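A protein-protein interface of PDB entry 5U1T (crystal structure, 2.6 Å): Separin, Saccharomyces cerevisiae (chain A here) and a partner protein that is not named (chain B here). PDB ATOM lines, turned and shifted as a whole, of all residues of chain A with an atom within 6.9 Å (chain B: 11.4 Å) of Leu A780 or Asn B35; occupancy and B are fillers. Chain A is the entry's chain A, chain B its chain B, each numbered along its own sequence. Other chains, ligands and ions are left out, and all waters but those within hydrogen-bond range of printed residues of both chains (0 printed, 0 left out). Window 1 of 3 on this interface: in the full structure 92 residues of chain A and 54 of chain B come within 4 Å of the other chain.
The backbone carbonyl oxygen (O) of Leu A774 sits at hydrogen-bond distance from the side-chain amino group (NZ) of Lys B30 (2.9 Å). O of Asn A778 lies within hydrogen-bond range of NZ of Lys B30, at 3.1 Å. The backbone carbonyl oxygen (O) of Leu A780 sits at hydrogen-bond distance from the side-chain amide nitrogen (ND2) of Asn B35, 2.4 Å away. O of Asn B35 lies close to N of Gln A782, at 3.5 Å. NH2 of Arg A785 is in hydrogen-bond range of O of Leu B31, at 2.7 Å. O of Lys B32 sits at hydrogen-bond distance from NH2 of Arg A785. The guanidinium group (NE) of Arg A785 sits close to the backbone carbonyl oxygen (O) of Thr B33 (3.3 Å). The backbone carbonyl oxygen of Lys A776 sits close to the side-chain amino group of Lys B30, at 2.3 Å.
The side-chain amide oxygen (OE1) of Gln A782 is in hydrogen-bond range of the guanidinium group (NH1) of Arg A785 (2.7 Å). OE1 of Glu B29 is in salt-bridge range of NZ of Lys B32 (3.5 Å). O of Glu B29 lies within hydrogen-bond range of OG1 of Thr B33. The backbone NH of Tyr B38 is in hydrogen-bond range of the side-chain hydroxyl of Ser B36 (2.8 Å).
Among the printed residues, pairs that only touch across the chains: Asn A567 with Pro B37, Gln A782 with Phe B34, Leu A774 with Asp B27, Lys A779 with Asn B35, Gly A534 with Ser B36, Leu A774 with Phe B23, Arg A785 with Lys B30, Leu A788 with Leu B31, Gly A534 with Phe B34, Arg A533 with Ser B36 and Leu A780 with Lys B30.
Of chain B, only Phe B34 and Ser B36 come within 4 Å of Gly A534. Leu A774 touches just these residues of chain B: Phe B23 (3.6 Å), Asp B27 (3.4 Å) and Lys B30 (2.9 Å). Of the printed residues of chain B, Lys A779 touches Asn B35. Leu A780 touches just these residues of chain B: Lys B30 and Asn B35. No residue of chain B comes within 4 Å of Ser A781. Gln A782 touches just these residues of chain B: Phe B34 (3.4 Å) and Asn B35 (3.3 Å). Ser A784 touches none of the printed residues of chain B. Arg A785 touches just these residues of chain B: Lys B30 (3.6 Å), Leu B31 (2.7 Å), Lys B32 (3.3 Å) and Thr B33 (3.2 Å). Printed residues of chain A within 4 Å of Phe B23: Leu A774. Asn B35 touches just these residues of chain A: Lys A779, Leu A780 and Gln A782.
Of the 19 printed residues of chain A, 11 touch a printed residue of chain B. Along chain A the printed residues that touch a printed residue of chain B span positions 533 to 788. Among the printed residues, 19 pairs touch across the chains. Among the printed residues, no Asp or Glu carboxylate lies within 4 Å of a Lys or Arg side-chain nitrogen of the other chain.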
ATOM      1  N   ARG A 533      38.072  -8.981   0.572  1.00  0.00           N
ATOM      2  CA  ARG A 533      38.023 -10.153  -0.302  1.00  0.00           C
ATOM      3  C   ARG A 533      36.673 -10.818  -0.434  1.00  0.00           C
ATOM      4  O   ARG A 533      36.476 -11.618  -1.333  1.00  0.00           O
ATOM      5  CB  ARG A 533      38.994 -11.210   0.190  1.00  0.00           C
ATOM      6  CG  ARG A 533      40.426 -10.828   0.065  1.00  0.00           C
ATOM      7  CD  ARG A 533      41.167 -12.037  -0.386  1.00  0.00           C
ATOM      8  NE  ARG A 533      41.605 -11.861  -1.755  1.00  0.00           N
ATOM      9  CZ  ARG A 533      42.242 -12.787  -2.450  1.00  0.00           C
ATOM     10  NH1 ARG A 533      42.510 -13.965  -1.907  1.00  0.00           N
ATOM     11  NH2 ARG A 533      42.606 -12.521  -3.690  1.00  0.00           N
ATOM     12  N   GLY A 534      35.765 -10.525   0.489  1.00  0.00           N
ATOM     13  CA  GLY A 534      34.506 -11.233   0.564  1.00  0.00           C
ATOM     14  C   GLY A 534      34.699 -12.672   0.993  1.00  0.00           C
ATOM     15  O   GLY A 534      33.904 -13.541   0.652  1.00  0.00           O
ATOM     16  N   ASN A 567      30.065  -7.498   6.485  1.00  0.00           N
ATOM     17  CA  ASN A 567      30.418  -8.301   5.325  1.00  0.00           C
ATOM     18  C   ASN A 567      30.351  -9.789   5.618  1.00  0.00           C
ATOM     19  O   ASN A 567      30.032 -10.570   4.732  1.00  0.00           O
ATOM     20  CB  ASN A 567      31.794  -7.906   4.804  1.00  0.00           C
ATOM     21  CG  ASN A 567      31.760  -6.622   4.003  1.00  0.00           C
ATOM     22  OD1 ASN A 567      31.853  -5.525   4.562  1.00  0.00           O
ATOM     23  ND2 ASN A 567      31.623  -6.747   2.685  1.00  0.00           N
ATOM     24  N   ILE A 733      25.799  -1.890 -15.543  1.00  0.00           N
ATOM     25  CA  ILE A 733      24.860  -2.722 -14.808  1.00  0.00           C
ATOM     26  C   ILE A 733      23.862  -1.839 -14.050  1.00  0.00           C
ATOM     27  O   ILE A 733      22.650  -2.115 -14.023  1.00  0.00           O
ATOM     28  CB  ILE A 733      25.586  -3.657 -13.823  1.00  0.00           C
ATOM     29  CG1 ILE A 733      26.441  -4.678 -14.568  1.00  0.00           C
ATOM     30  CG2 ILE A 733      24.596  -4.379 -12.927  1.00  0.00           C
ATOM     31  CD1 ILE A 733      25.657  -5.698 -15.318  1.00  0.00           C
ATOM     32  N   LEU A 737      19.751  -1.523 -14.353  1.00  0.00           N
ATOM     33  CA  LEU A 737      18.929  -1.612 -13.147  1.00  0.00           C
ATOM     34  C   LEU A 737      18.009  -0.400 -12.985  1.00  0.00           C
ATOM     35  O   LEU A 737      16.886  -0.542 -12.512  1.00  0.00           O
ATOM     36  CB  LEU A 737      19.801  -1.761 -11.903  1.00  0.00           C
ATOM     37  CG  LEU A 737      20.552  -3.081 -11.745  1.00  0.00           C
ATOM     38  CD1 LEU A 737      21.529  -2.985 -10.582  1.00  0.00           C
ATOM     39  CD2 LEU A 737      19.604  -4.248 -11.554  1.00  0.00           C
ATOM     40  N   LEU A 773      20.563  -8.460 -18.284  1.00  0.00           N
ATOM     41  CA  LEU A 773      21.503  -7.968 -17.297  1.00  0.00           C
ATOM     42  C   LEU A 773      22.281  -9.116 -16.711  1.00  0.00           C
ATOM     43  O   LEU A 773      23.427  -8.975 -16.364  1.00  0.00           O
ATOM     44  CB  LEU A 773      20.767  -7.254 -16.189  1.00  0.00           C
ATOM     45  CG  LEU A 773      21.611  -6.503 -15.186  1.00  0.00           C
ATOM     46  CD1 LEU A 773      20.776  -5.420 -14.566  1.00  0.00           C
ATOM     47  CD2 LEU A 773      22.091  -7.438 -14.117  1.00  0.00           C
ATOM     48  N   LEU A 774      21.658 -10.270 -16.609  1.00  0.00           N
ATOM     49  CA  LEU A 774      22.321 -11.429 -16.084  1.00  0.00           C
ATOM     50  C   LEU A 774      23.250 -12.053 -17.089  1.00  0.00           C
ATOM     51  O   LEU A 774      24.150 -12.766 -16.723  1.00  0.00           O
ATOM     52  CB  LEU A 774      21.299 -12.468 -15.686  1.00  0.00           C
ATOM     53  CG  LEU A 774      20.414 -12.079 -14.529  1.00  0.00           C
ATOM     54  CD1 LEU A 774      19.354 -13.125 -14.332  1.00  0.00           C
ATOM     55  CD2 LEU A 774      21.227 -11.915 -13.270  1.00  0.00           C
ATOM     56  N   LYS A 776      25.245 -10.394 -19.037  1.00  0.00           N
ATOM     57  CA  LYS A 776      26.461  -9.622 -19.085  1.00  0.00           C
ATOM     58  C   LYS A 776      27.524 -10.404 -18.342  1.00  0.00           C
ATOM     59  O   LYS A 776      27.290 -10.920 -17.264  1.00  0.00           O
ATOM     60  CB  LYS A 776      26.267  -8.309 -18.355  1.00  0.00           C
ATOM     61  CG  LYS A 776      25.884  -7.138 -19.225  1.00  0.00           C
ATOM     62  CD  LYS A 776      25.199  -7.570 -20.496  1.00  0.00           C
ATOM     63  CE  LYS A 776      24.293  -6.476 -21.007  1.00  0.00           C
ATOM     64  NZ  LYS A 776      23.940  -6.734 -22.417  1.00  0.00           N
ATOM     65  N   LYS A 777      28.749 -10.395 -18.839  1.00  0.00           N
ATOM     66  CA  LYS A 777      29.846 -11.143 -18.223  1.00  0.00           C
ATOM     67  C   LYS A 777      30.270 -10.827 -16.786  1.00  0.00           C
ATOM     68  O   LYS A 777      30.970 -11.606 -16.179  1.00  0.00           O
ATOM     69  CB  LYS A 777      31.062 -11.130 -19.128  1.00  0.00           C
ATOM     70  CG  LYS A 777      31.010 -12.210 -20.193  1.00  0.00           C
ATOM     71  CD  LYS A 777      31.886 -11.849 -21.381  1.00  0.00           C
ATOM     72  CE  LYS A 777      31.115 -11.885 -22.692  1.00  0.00           C
ATOM     73  NZ  LYS A 777      31.450 -10.744 -23.592  1.00  0.00           N
ATOM     74  N   ASN A 778      29.861  -9.691 -16.260  1.00  0.00           N
ATOM     75  CA  ASN A 778      30.113  -9.242 -14.913  1.00  0.00           C
ATOM     76  C   ASN A 778      30.023 -10.251 -13.786  1.00  0.00           C
ATOM     77  O   ASN A 778      29.189 -11.127 -13.775  1.00  0.00           O
ATOM     78  CB  ASN A 778      29.035  -8.204 -14.625  1.00  0.00           C
ATOM     79  CG  ASN A 778      29.353  -7.338 -13.441  1.00  0.00           C
ATOM     80  OD1 ASN A 778      28.478  -6.973 -12.675  1.00  0.00           O
ATOM     81  ND2 ASN A 778      30.618  -7.016 -13.280  1.00  0.00           N
ATOM     82  N   LYS A 779      30.872 -10.058 -12.802  1.00  0.00           N
ATOM     83  CA  LYS A 779      30.815 -10.841 -11.607  1.00  0.00           C
ATOM     84  C   LYS A 779      29.997  -9.873 -10.791  1.00  0.00           C
ATOM     85  O   LYS A 779      30.535  -8.989 -10.165  1.00  0.00           O
ATOM     86  CB  LYS A 779      32.192 -11.003 -11.001  1.00  0.00           C
ATOM     87  CG  LYS A 779      33.137 -11.831 -11.840  1.00  0.00           C
ATOM     88  CD  LYS A 779      34.509 -11.940 -11.200  1.00  0.00           C
ATOM     89  CE  LYS A 779      35.451 -12.793 -12.032  1.00  0.00           C
ATOM     90  NZ  LYS A 779      36.801 -12.878 -11.412  1.00  0.00           N
ATOM     91  N   LEU A 780      28.688 -10.025 -10.834  1.00  0.00           N
ATOM     92  CA  LEU A 780      27.760  -9.133 -10.151  1.00  0.00           C
ATOM     93  C   LEU A 780      28.144  -8.655  -8.770  1.00  0.00           C
ATOM     94  O   LEU A 780      28.394  -9.454  -7.907  1.00  0.00           O
ATOM     95  CB  LEU A 780      26.423  -9.838 -10.064  1.00  0.00           C
ATOM     96  CG  LEU A 780      25.175  -8.990 -10.070  1.00  0.00           C
ATOM     97  CD1 LEU A 780      25.404  -7.733 -10.863  1.00  0.00           C
ATOM     98  CD2 LEU A 780      24.045  -9.786 -10.661  1.00  0.00           C
ATOM     99  N   SER A 781      28.143  -7.348  -8.555  1.00  0.00           N
ATOM    100  CA  SER A 781      28.499  -6.790  -7.245  1.00  0.00           C
ATOM    101  C   SER A 781      27.356  -6.929  -6.244  1.00  0.00           C
ATOM    102  O   SER A 781      26.202  -6.810  -6.610  1.00  0.00           O
ATOM    103  CB  SER A 781      28.905  -5.322  -7.364  1.00  0.00           C
ATOM    104  OG  SER A 781      27.781  -4.456  -7.416  1.00  0.00           O
ATOM    105  N   GLN A 782      27.691  -7.165  -4.981  1.00  0.00           N
ATOM    106  CA  GLN A 782      26.698  -7.319  -3.934  1.00  0.00           C
ATOM    107  C   GLN A 782      25.572  -6.302  -4.020  1.00  0.00           C
ATOM    108  O   GLN A 782      24.411  -6.692  -4.020  1.00  0.00           O
ATOM    109  CB  GLN A 782      27.346  -7.220  -2.558  1.00  0.00           C
ATOM    110  CG  GLN A 782      26.345  -7.131  -1.403  1.00  0.00           C
ATOM    111  CD  GLN A 782      25.673  -8.460  -1.072  1.00  0.00           C
ATOM    112  OE1 GLN A 782      25.504  -9.329  -1.930  1.00  0.00           O
ATOM    113  NE2 GLN A 782      25.291  -8.622   0.183  1.00  0.00           N
ATOM    114  N   GLY A 783      25.907  -5.015  -4.108  1.00  0.00           N
ATOM    115  CA  GLY A 783      24.904  -3.958  -4.190  1.00  0.00           C
ATOM    116  C   GLY A 783      23.949  -4.102  -5.373  1.00  0.00           C
ATOM    117  O   GLY A 783      22.729  -3.924  -5.253  1.00  0.00           O
ATOM    118  N   SER A 784      24.497  -4.443  -6.527  1.00  0.00           N
ATOM    119  CA  SER A 784      23.682  -4.664  -7.699  1.00  0.00           C
ATOM    120  C   SER A 784      22.916  -5.990  -7.637  1.00  0.00           C
ATOM    121  O   SER A 784      21.843  -6.103  -8.202  1.00  0.00           O
ATOM    122  CB  SER A 784      24.553  -4.608  -8.948  1.00  0.00           C
ATOM    123  OG  SER A 784      24.671  -3.267  -9.366  1.00  0.00           O
ATOM    124  N   ARG A 785      23.457  -6.993  -6.957  1.00  0.00           N
ATOM    125  CA  ARG A 785      22.770  -8.271  -6.876  1.00  0.00           C
ATOM    126  C   ARG A 785      21.501  -8.107  -6.039  1.00  0.00           C
ATOM    127  O   ARG A 785      20.456  -8.669  -6.359  1.00  0.00           O
ATOM    128  CB  ARG A 785      23.680  -9.353  -6.292  1.00  0.00           C
ATOM    129  CG  ARG A 785      23.042 -10.712  -6.265  1.00  0.00           C
ATOM    130  CD  ARG A 785      23.951 -11.728  -5.663  1.00  0.00           C
ATOM    131  NE  ARG A 785      24.286 -11.432  -4.283  1.00  0.00           N
ATOM    132  CZ  ARG A 785      23.693 -11.991  -3.235  1.00  0.00           C
ATOM    133  NH1 ARG A 785      24.066 -11.664  -2.008  1.00  0.00           N
ATOM    134  NH2 ARG A 785      22.725 -12.878  -3.404  1.00  0.00           N
ATOM    135  N   LEU A 786      21.602  -7.319  -4.973  1.00  0.00           N
ATOM    136  CA  LEU A 786      20.477  -7.078  -4.101  1.00  0.00           C
ATOM    137  C   LEU A 786      19.461  -6.221  -4.827  1.00  0.00           C
ATOM    138  O   LEU A 786      18.265  -6.431  -4.685  1.00  0.00           O
ATOM    139  CB  LEU A 786      20.923  -6.403  -2.796  1.00  0.00           C
ATOM    140  CG  LEU A 786      21.929  -7.150  -1.922  1.00  0.00           C
ATOM    141  CD1 LEU A 786      22.357  -6.293  -0.741  1.00  0.00           C
ATOM    142  CD2 LEU A 786      21.402  -8.505  -1.463  1.00  0.00           C
ATOM    143  N   LEU A 788      18.817  -6.142  -7.985  1.00  0.00           N
ATOM    144  CA  LEU A 788      18.196  -7.025  -8.950  1.00  0.00           C
ATOM    145  C   LEU A 788      17.263  -8.037  -8.291  1.00  0.00           C
ATOM    146  O   LEU A 788      16.297  -8.478  -8.897  1.00  0.00           O
ATOM    147  CB  LEU A 788      19.281  -7.750  -9.736  1.00  0.00           C
ATOM    148  CG  LEU A 788      18.791  -8.652 -10.851  1.00  0.00           C
ATOM    149  CD1 LEU A 788      17.974  -7.824 -11.816  1.00  0.00           C
ATOM    150  CD2 LEU A 788      19.995  -9.254 -11.534  1.00  0.00           C
ATOM    151  N   PHE B  23      14.245 -17.857 -16.374  1.00  0.00           N
ATOM    152  CA  PHE B  23      15.581 -17.625 -15.863  1.00  0.00           C
ATOM    153  C   PHE B  23      16.324 -18.947 -15.786  1.00  0.00           C
ATOM    154  O   PHE B  23      15.870 -19.902 -15.160  1.00  0.00           O
ATOM    155  CB  PHE B  23      15.514 -16.907 -14.513  1.00  0.00           C
ATOM    156  CG  PHE B  23      15.108 -15.468 -14.645  1.00  0.00           C
ATOM    157  CD1 PHE B  23      13.758 -15.124 -14.841  1.00  0.00           C
ATOM    158  CD2 PHE B  23      16.068 -14.461 -14.654  1.00  0.00           C
ATOM    159  CE1 PHE B  23      13.371 -13.792 -15.010  1.00  0.00           C
ATOM    160  CE2 PHE B  23      15.705 -13.128 -14.818  1.00  0.00           C
ATOM    161  CZ  PHE B  23      14.353 -12.785 -14.997  1.00  0.00           C
ATOM    162  N   ASP B  26      22.150 -20.859 -14.687  1.00  0.00           N
ATOM    163  CA  ASP B  26      23.251 -19.893 -14.584  1.00  0.00           C
ATOM    164  C   ASP B  26      22.809 -18.583 -13.956  1.00  0.00           C
ATOM    165  O   ASP B  26      23.419 -18.091 -13.012  1.00  0.00           O
ATOM    166  CB  ASP B  26      23.846 -19.608 -15.962  1.00  0.00           C
ATOM    167  CG  ASP B  26      24.943 -20.582 -16.325  1.00  0.00           C
ATOM    168  OD1 ASP B  26      25.115 -21.558 -15.555  1.00  0.00           O
ATOM    169  OD2 ASP B  26      25.625 -20.386 -17.371  1.00  0.00           O
ATOM    170  N   ASP B  27      21.741 -18.025 -14.512  1.00  0.00           N
ATOM    171  CA  ASP B  27      21.139 -16.800 -14.012  1.00  0.00           C
ATOM    172  C   ASP B  27      20.871 -16.895 -12.503  1.00  0.00           C
ATOM    173  O   ASP B  27      21.108 -15.945 -11.760  1.00  0.00           O
ATOM    174  CB  ASP B  27      19.846 -16.505 -14.789  1.00  0.00           C
ATOM    175  CG  ASP B  27      20.032 -16.613 -16.307  1.00  0.00           C
ATOM    176  OD1 ASP B  27      21.192 -16.582 -16.773  1.00  0.00           O
ATOM    177  OD2 ASP B  27      19.023 -16.731 -17.039  1.00  0.00           O
ATOM    178  N   ILE B  28      20.406 -18.056 -12.053  1.00  0.00           N
ATOM    179  CA  ILE B  28      20.053 -18.248 -10.648  1.00  0.00           C
ATOM    180  C   ILE B  28      21.312 -18.220  -9.782  1.00  0.00           C
ATOM    181  O   ILE B  28      21.303 -17.652  -8.693  1.00  0.00           O
ATOM    182  CB  ILE B  28      19.247 -19.577 -10.424  1.00  0.00           C
ATOM    183  CG1 ILE B  28      17.767 -19.362 -10.749  1.00  0.00           C
ATOM    184  CG2 ILE B  28      19.386 -20.095  -8.993  1.00  0.00           C
ATOM    185  CD1 ILE B  28      16.829 -20.415 -10.137  1.00  0.00           C
ATOM    186  N   GLU B  29      22.399 -18.809 -10.270  1.00  0.00           N
ATOM    187  CA  GLU B  29      23.646 -18.789  -9.515  1.00  0.00           C
ATOM    188  C   GLU B  29      24.117 -17.354  -9.328  1.00  0.00           C
ATOM    189  O   GLU B  29      24.531 -16.963  -8.239  1.00  0.00           O
ATOM    190  CB  GLU B  29      24.721 -19.632 -10.201  1.00  0.00           C
ATOM    191  CG  GLU B  29      24.403 -21.138 -10.261  1.00  0.00           C
ATOM    192  CD  GLU B  29      24.177 -21.768  -8.876  1.00  0.00           C
ATOM    193  OE1 GLU B  29      24.917 -21.416  -7.920  1.00  0.00           O
ATOM    194  OE2 GLU B  29      23.263 -22.621  -8.741  1.00  0.00           O
ATOM    195  N   LYS B  30      24.012 -16.564 -10.385  1.00  0.00           N
ATOM    196  CA  LYS B  30      24.400 -15.166 -10.350  1.00  0.00           C
ATOM    197  C   LYS B  30      23.565 -14.358  -9.340  1.00  0.00           C
ATOM    198  O   LYS B  30      23.984 -13.297  -8.912  1.00  0.00           O
ATOM    199  CB  LYS B  30      24.272 -14.578 -11.755  1.00  0.00           C
ATOM    200  CG  LYS B  30      25.073 -13.325 -12.051  1.00  0.00           C
ATOM    201  CD  LYS B  30      25.675 -13.420 -13.458  1.00  0.00           C
ATOM    202  CE  LYS B  30      26.081 -12.064 -14.022  1.00  0.00           C
ATOM    203  NZ  LYS B  30      26.711 -12.169 -15.393  1.00  0.00           N
ATOM    204  N   LEU B  31      22.393 -14.859  -8.958  1.00  0.00           N
ATOM    205  CA  LEU B  31      21.525 -14.153  -8.010  1.00  0.00           C
ATOM    206  C   LEU B  31      21.771 -14.588  -6.562  1.00  0.00           C
ATOM    207  O   LEU B  31      21.504 -13.835  -5.624  1.00  0.00           O
ATOM    208  CB  LEU B  31      20.039 -14.365  -8.370  1.00  0.00           C
ATOM    209  CG  LEU B  31      19.557 -13.873  -9.744  1.00  0.00           C
ATOM    210  CD1 LEU B  31      18.379 -14.674 -10.259  1.00  0.00           C
ATOM    211  CD2 LEU B  31      19.217 -12.400  -9.723  1.00  0.00           C
ATOM    212  N   LYS B  32      22.267 -15.810  -6.392  1.00  0.00           N
ATOM    213  CA  LYS B  32      22.536 -16.381  -5.071  1.00  0.00           C
ATOM    214  C   LYS B  32      23.862 -15.913  -4.521  1.00  0.00           C
ATOM    215  O   LYS B  32      24.075 -15.910  -3.307  1.00  0.00           O
ATOM    216  CB  LYS B  32      22.559 -17.911  -5.126  1.00  0.00           C
ATOM    217  CG  LYS B  32      21.212 -18.572  -5.345  1.00  0.00           C
ATOM    218  CD  LYS B  32      21.406 -20.040  -5.706  1.00  0.00           C
ATOM    219  CE  LYS B  32      22.202 -20.763  -4.631  1.00  0.00           C
ATOM    220  NZ  LYS B  32      22.829 -22.009  -5.175  1.00  0.00           N
ATOM    221  N   THR B  33      24.753 -15.515  -5.422  1.00  0.00           N
ATOM    222  CA  THR B  33      26.176 -15.492  -5.122  1.00  0.00           C
ATOM    223  C   THR B  33      26.743 -14.156  -4.662  1.00  0.00           C
ATOM    224  O   THR B  33      26.805 -13.170  -5.399  1.00  0.00           O
ATOM    225  CB  THR B  33      26.960 -15.978  -6.347  1.00  0.00           C
ATOM    226  OG1 THR B  33      26.729 -17.383  -6.501  1.00  0.00           O
ATOM    227  CG2 THR B  33      28.457 -15.711  -6.183  1.00  0.00           C
ATOM    228  N   PHE B  34      27.185 -14.164  -3.414  1.00  0.00           N
ATOM    229  CA  PHE B  34      27.857 -13.025  -2.823  1.00  0.00           C
ATOM    230  C   PHE B  34      29.251 -12.748  -3.439  1.00  0.00           C
ATOM    231  O   PHE B  34      30.073 -13.645  -3.587  1.00  0.00           O
ATOM    232  CB  PHE B  34      27.977 -13.243  -1.319  1.00  0.00           C
ATOM    233  CG  PHE B  34      28.721 -12.151  -0.613  1.00  0.00           C
ATOM    234  CD1 PHE B  34      28.119 -10.923  -0.378  1.00  0.00           C
ATOM    235  CD2 PHE B  34      30.033 -12.349  -0.194  1.00  0.00           C
ATOM    236  CE1 PHE B  34      28.816  -9.908   0.255  1.00  0.00           C
ATOM    237  CE2 PHE B  34      30.736 -11.339   0.444  1.00  0.00           C
ATOM    238  CZ  PHE B  34      30.132 -10.117   0.672  1.00  0.00           C
ATOM    239  N   ASN B  35      29.475 -11.491  -3.822  1.00  0.00           N
ATOM    240  CA  ASN B  35      30.781 -10.970  -4.216  1.00  0.00           C
ATOM    241  C   ASN B  35      31.050  -9.727  -3.401  1.00  0.00           C
ATOM    242  O   ASN B  35      30.127  -8.934  -3.204  1.00  0.00           O
ATOM    243  CB  ASN B  35      30.828 -10.599  -5.681  1.00  0.00           C
ATOM    244  CG  ASN B  35      30.463 -11.729  -6.571  1.00  0.00           C
ATOM    245  OD1 ASN B  35      30.772 -12.878  -6.287  1.00  0.00           O
ATOM    246  ND2 ASN B  35      29.802 -11.415  -7.670  1.00  0.00           N
ATOM    247  N   SER B  36      32.282  -9.545  -2.929  1.00  0.00           N
ATOM    248  CA  SER B  36      32.596  -8.417  -2.073  1.00  0.00           C
ATOM    249  C   SER B  36      32.236  -7.091  -2.706  1.00  0.00           C
ATOM    250  O   SER B  36      32.605  -6.824  -3.848  1.00  0.00           O
ATOM    251  CB  SER B  36      34.079  -8.394  -1.725  1.00  0.00           C
ATOM    252  OG  SER B  36      34.489  -7.071  -1.422  1.00  0.00           O
ATOM    253  N   PRO B  37      31.543  -6.236  -1.941  1.00  0.00           N
ATOM    254  CA  PRO B  37      31.270  -4.859  -2.363  1.00  0.00           C
ATOM    255  C   PRO B  37      32.550  -4.092  -2.659  1.00  0.00           C
ATOM    256  O   PRO B  37      32.485  -3.087  -3.363  1.00  0.00           O
ATOM    257  CB  PRO B  37      30.554  -4.257  -1.157  1.00  0.00           C
ATOM    258  CG  PRO B  37      31.033  -5.075   0.009  1.00  0.00           C
ATOM    259  CD  PRO B  37      31.149  -6.475  -0.542  1.00  0.00           C
ATOM    260  N   TYR B  38      33.664  -4.518  -2.091  1.00  0.00           N
ATOM    261  CA  TYR B  38      34.930  -3.804  -2.227  1.00  0.00           C
ATOM    262  C   TYR B  38      35.715  -4.054  -3.492  1.00  0.00           C
ATOM    263  O   TYR B  38      36.667  -3.364  -3.759  1.00  0.00           O
ATOM    264  CB  TYR B  38      35.833  -4.099  -1.037  1.00  0.00           C
ATOM    265  CG  TYR B  38      35.526  -3.326   0.200  1.00  0.00           C
ATOM    266  CD1 TYR B  38      35.832  -2.000   0.292  1.00  0.00           C
ATOM    267  CD2 TYR B  38      34.943  -3.929   1.281  1.00  0.00           C
ATOM    268  CE1 TYR B  38      35.551  -1.289   1.424  1.00  0.00           C
ATOM    269  CE2 TYR B  38      34.664  -3.222   2.415  1.00  0.00           C
ATOM    270  CZ  TYR B  38      34.973  -1.902   2.473  1.00  0.00           C
ATOM    271  OH  TYR B  38      34.706  -1.176   3.585  1.00  0.00           O
ATOM    272  N   LYS B  39      35.356  -5.070  -4.234  1.00  0.00           N
ATOM    273  CA  LYS B  39      36.060  -5.342  -5.444  1.00  0.00           C
ATOM    274  C   LYS B  39      35.817  -4.200  -6.372  1.00  0.00           C
ATOM    275  O   LYS B  39      34.726  -3.710  -6.480  1.00  0.00           O
ATOM    276  CB  LYS B  39      35.528  -6.605  -6.093  1.00  0.00           C
ATOM    277  CG  LYS B  39      36.143  -7.884  -5.579  1.00  0.00           C
ATOM    278  CD  LYS B  39      35.296  -9.089  -5.940  1.00  0.00           C
ATOM    279  CE  LYS B  39      35.595 -10.287  -5.058  1.00  0.00           C
ATOM    280  NZ  LYS B  39      34.686 -11.434  -5.332  1.00  0.00           N
ATOM    281  N   LEU B  40      36.855  -3.749  -7.031  1.00  0.00           N
ATOM    282  CA  LEU B  40      36.716  -2.697  -8.008  1.00  0.00           C
ATOM    283  C   LEU B  40      37.281  -3.128  -9.349  1.00  0.00           C
ATOM    284  O   LEU B  40      37.894  -4.178  -9.462  1.00  0.00           O
ATOM    285  CB  LEU B  40      37.354  -1.409  -7.525  1.00  0.00           C
ATOM    286  CG  LEU B  40      38.836  -1.333  -7.269  1.00  0.00           C
ATOM    287  CD1 LEU B  40      39.062  -0.235  -6.262  1.00  0.00           C
ATOM    288  CD2 LEU B  40      39.329  -2.649  -6.730  1.00  0.00           C
ATOM    289  N   ASP B  41      37.057  -2.336 -10.384  1.00  0.00           N
ATOM    290  CA  ASP B  41      37.582  -2.703 -11.698  1.00  0.00           C
ATOM    291  C   ASP B  41      37.923  -1.533 -12.590  1.00  0.00           C
ATOM    292  O   ASP B  41      37.094  -0.673 -12.828  1.00  0.00           O
ATOM    293  CB  ASP B  41      36.627  -3.638 -12.428  1.00  0.00           C
ATOM    294  CG  ASP B  41      37.335  -4.503 -13.435  1.00  0.00           C
ATOM    295  OD1 ASP B  41      38.080  -3.951 -14.261  1.00  0.00           O
ATOM    296  OD2 ASP B  41      37.162  -5.734 -13.394  1.00  0.00           O
